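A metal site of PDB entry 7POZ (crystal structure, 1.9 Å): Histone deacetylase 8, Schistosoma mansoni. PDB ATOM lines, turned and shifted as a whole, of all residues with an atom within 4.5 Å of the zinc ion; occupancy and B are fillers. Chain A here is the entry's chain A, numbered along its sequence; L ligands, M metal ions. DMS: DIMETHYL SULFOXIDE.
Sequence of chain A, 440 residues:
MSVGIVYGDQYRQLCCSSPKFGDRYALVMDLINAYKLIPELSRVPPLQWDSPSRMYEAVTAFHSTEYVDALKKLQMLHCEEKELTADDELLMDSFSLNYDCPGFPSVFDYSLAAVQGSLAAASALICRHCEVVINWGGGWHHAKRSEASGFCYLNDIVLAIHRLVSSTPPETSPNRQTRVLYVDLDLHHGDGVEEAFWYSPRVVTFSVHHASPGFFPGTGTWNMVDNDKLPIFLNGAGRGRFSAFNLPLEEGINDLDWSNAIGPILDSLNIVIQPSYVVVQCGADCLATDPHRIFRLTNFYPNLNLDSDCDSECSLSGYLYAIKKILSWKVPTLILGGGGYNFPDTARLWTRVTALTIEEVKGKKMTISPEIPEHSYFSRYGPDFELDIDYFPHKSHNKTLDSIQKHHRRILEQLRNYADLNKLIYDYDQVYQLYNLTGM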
ATOM      1  N   ASP A 186      28.729   3.857 -13.423  1.00  0.00           N
ATOM      2  CA  ASP A 186      27.804   4.873 -12.837  1.00  0.00           C
ATOM      3  C   ASP A 186      27.527   4.521 -11.374  1.00  0.00           C
ATOM      4  O   ASP A 186      27.590   3.339 -11.035  1.00  0.00           O
ATOM      5  CB  ASP A 186      26.518   4.906 -13.651  1.00  0.00           C
ATOM      6  CG  ASP A 186      25.628   6.104 -13.398  1.00  0.00           C
ATOM      7  OD1 ASP A 186      24.887   6.072 -12.393  1.00  0.00           O
ATOM      8  OD2 ASP A 186      25.642   7.017 -14.251  1.00  0.00           O
ATOM      9  N   LEU A 187      27.247   5.524 -10.531  1.00  0.00           N
ATOM     10  CA  LEU A 187      26.801   5.317  -9.135  1.00  0.00           C
ATOM     11  C   LEU A 187      25.596   4.379  -9.110  1.00  0.00           C
ATOM     12  O   LEU A 187      25.431   3.648  -8.126  1.00  0.00           O
ATOM     13  CB  LEU A 187      26.436   6.670  -8.531  1.00  0.00           C
ATOM     14  CG  LEU A 187      25.975   6.641  -7.074  1.00  0.00           C
ATOM     15  CD1 LEU A 187      27.092   6.136  -6.173  1.00  0.00           C
ATOM     16  CD2 LEU A 187      25.501   8.017  -6.641  1.00  0.00           C
ATOM     17  N   HIS A 188      24.747   4.432 -10.145  1.00  0.00           N
ATOM     18  CA  HIS A 188      23.463   3.684 -10.160  1.00  0.00           C
ATOM     19  C   HIS A 188      23.609   2.402 -10.955  1.00  0.00           C
ATOM     20  O   HIS A 188      24.397   2.401 -11.894  1.00  0.00           O
ATOM     21  CB  HIS A 188      22.317   4.533 -10.705  1.00  0.00           C
ATOM     22  CG  HIS A 188      22.073   5.777  -9.928  1.00  0.00           C
ATOM     23  ND1 HIS A 188      22.698   6.973 -10.220  1.00  0.00           N
ATOM     24  CD2 HIS A 188      21.269   6.023  -8.862  1.00  0.00           C
ATOM     25  CE1 HIS A 188      22.267   7.914  -9.390  1.00  0.00           C
ATOM     26  NE2 HIS A 188      21.392   7.350  -8.539  1.00  0.00           N
ATOM     27  N   ASP A 285      28.879  10.200 -11.306  1.00  0.00           N
ATOM     28  CA  ASP A 285      28.172  10.522 -10.041  1.00  0.00           C
ATOM     29  C   ASP A 285      28.785   9.737  -8.871  1.00  0.00           C
ATOM     30  O   ASP A 285      28.249   9.856  -7.769  1.00  0.00           O
ATOM     31  CB  ASP A 285      26.654  10.367 -10.143  1.00  0.00           C
ATOM     32  CG  ASP A 285      26.162   9.172 -10.933  1.00  0.00           C
ATOM     33  OD1 ASP A 285      27.009   8.373 -11.392  1.00  0.00           O
ATOM     34  OD2 ASP A 285      24.914   9.037 -11.065  1.00  0.00           O
ATOM     35  N   GLY A 339      25.258   9.551 -15.688  1.00  0.00           N
ATOM     36  CA  GLY A 339      25.086  10.415 -14.507  1.00  0.00           C
ATOM     37  C   GLY A 339      26.266  11.338 -14.322  1.00  0.00           C
ATOM     38  O   GLY A 339      27.278  11.160 -15.036  1.00  0.00           O
ATOM     39  N   TYR A 341      26.280  15.128 -11.840  1.00  0.00           N
ATOM     40  CA  TYR A 341      25.333  16.214 -11.488  1.00  0.00           C
ATOM     41  C   TYR A 341      26.108  17.453 -10.997  1.00  0.00           C
ATOM     42  O   TYR A 341      25.511  18.530 -10.933  1.00  0.00           O
ATOM     43  CB  TYR A 341      24.285  15.628 -10.546  1.00  0.00           C
ATOM     44  CG  TYR A 341      23.593  14.462 -11.184  1.00  0.00           C
ATOM     45  CD1 TYR A 341      22.619  14.657 -12.158  1.00  0.00           C
ATOM     46  CD2 TYR A 341      23.956  13.155 -10.886  1.00  0.00           C
ATOM     47  CE1 TYR A 341      22.002  13.587 -12.779  1.00  0.00           C
ATOM     48  CE2 TYR A 341      23.349  12.079 -11.517  1.00  0.00           C
ATOM     49  CZ  TYR A 341      22.364  12.290 -12.467  1.00  0.00           C
ATOM     50  OH  TYR A 341      21.746  11.230 -13.074  1.00  0.00           O
HETATM   51  S   DMS L   1      21.695   8.346 -13.543  1.00  0.00           S
HETATM   52  O   DMS L   1      22.888   8.978 -12.883  1.00  0.00           O
HETATM   53  C1  DMS L   1      22.123   6.676 -13.706  1.00  0.00           C
HETATM   54  C2  DMS L   1      21.752   8.772 -15.264  1.00  0.00           C
HETATM   55 ZN    ZN M   1      23.807   7.624 -11.881  1.00  0.00          ZN
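The side-chain carboxylate of Asp 285 sits at hydrogen-bond distance from the backbone NH of Leu 187, at 3.0 Å.
OD2 of Asp 186 lies within hydrogen-bond range of N of Gly 339, 2.9 Å away.
Three residues have an atom within 4 Å of the zinc ion: Asp 186, His 188 and Asp 285.
Along chain A the residues within 4 Å of the zinc ion span positions 186 to 285.
The nearest printed residue that does not touch the zinc ion is Gly 339 (4.04 Å).
The zinc ion is bound by O of the ligand (1.9 Å), OD1 of Asp 186 (2.0 Å), OD2 of Asp 285 (2.0 Å) and ND1 of His 188 (2.1 Å).
The zinc ion has four donor atoms within binding distance.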
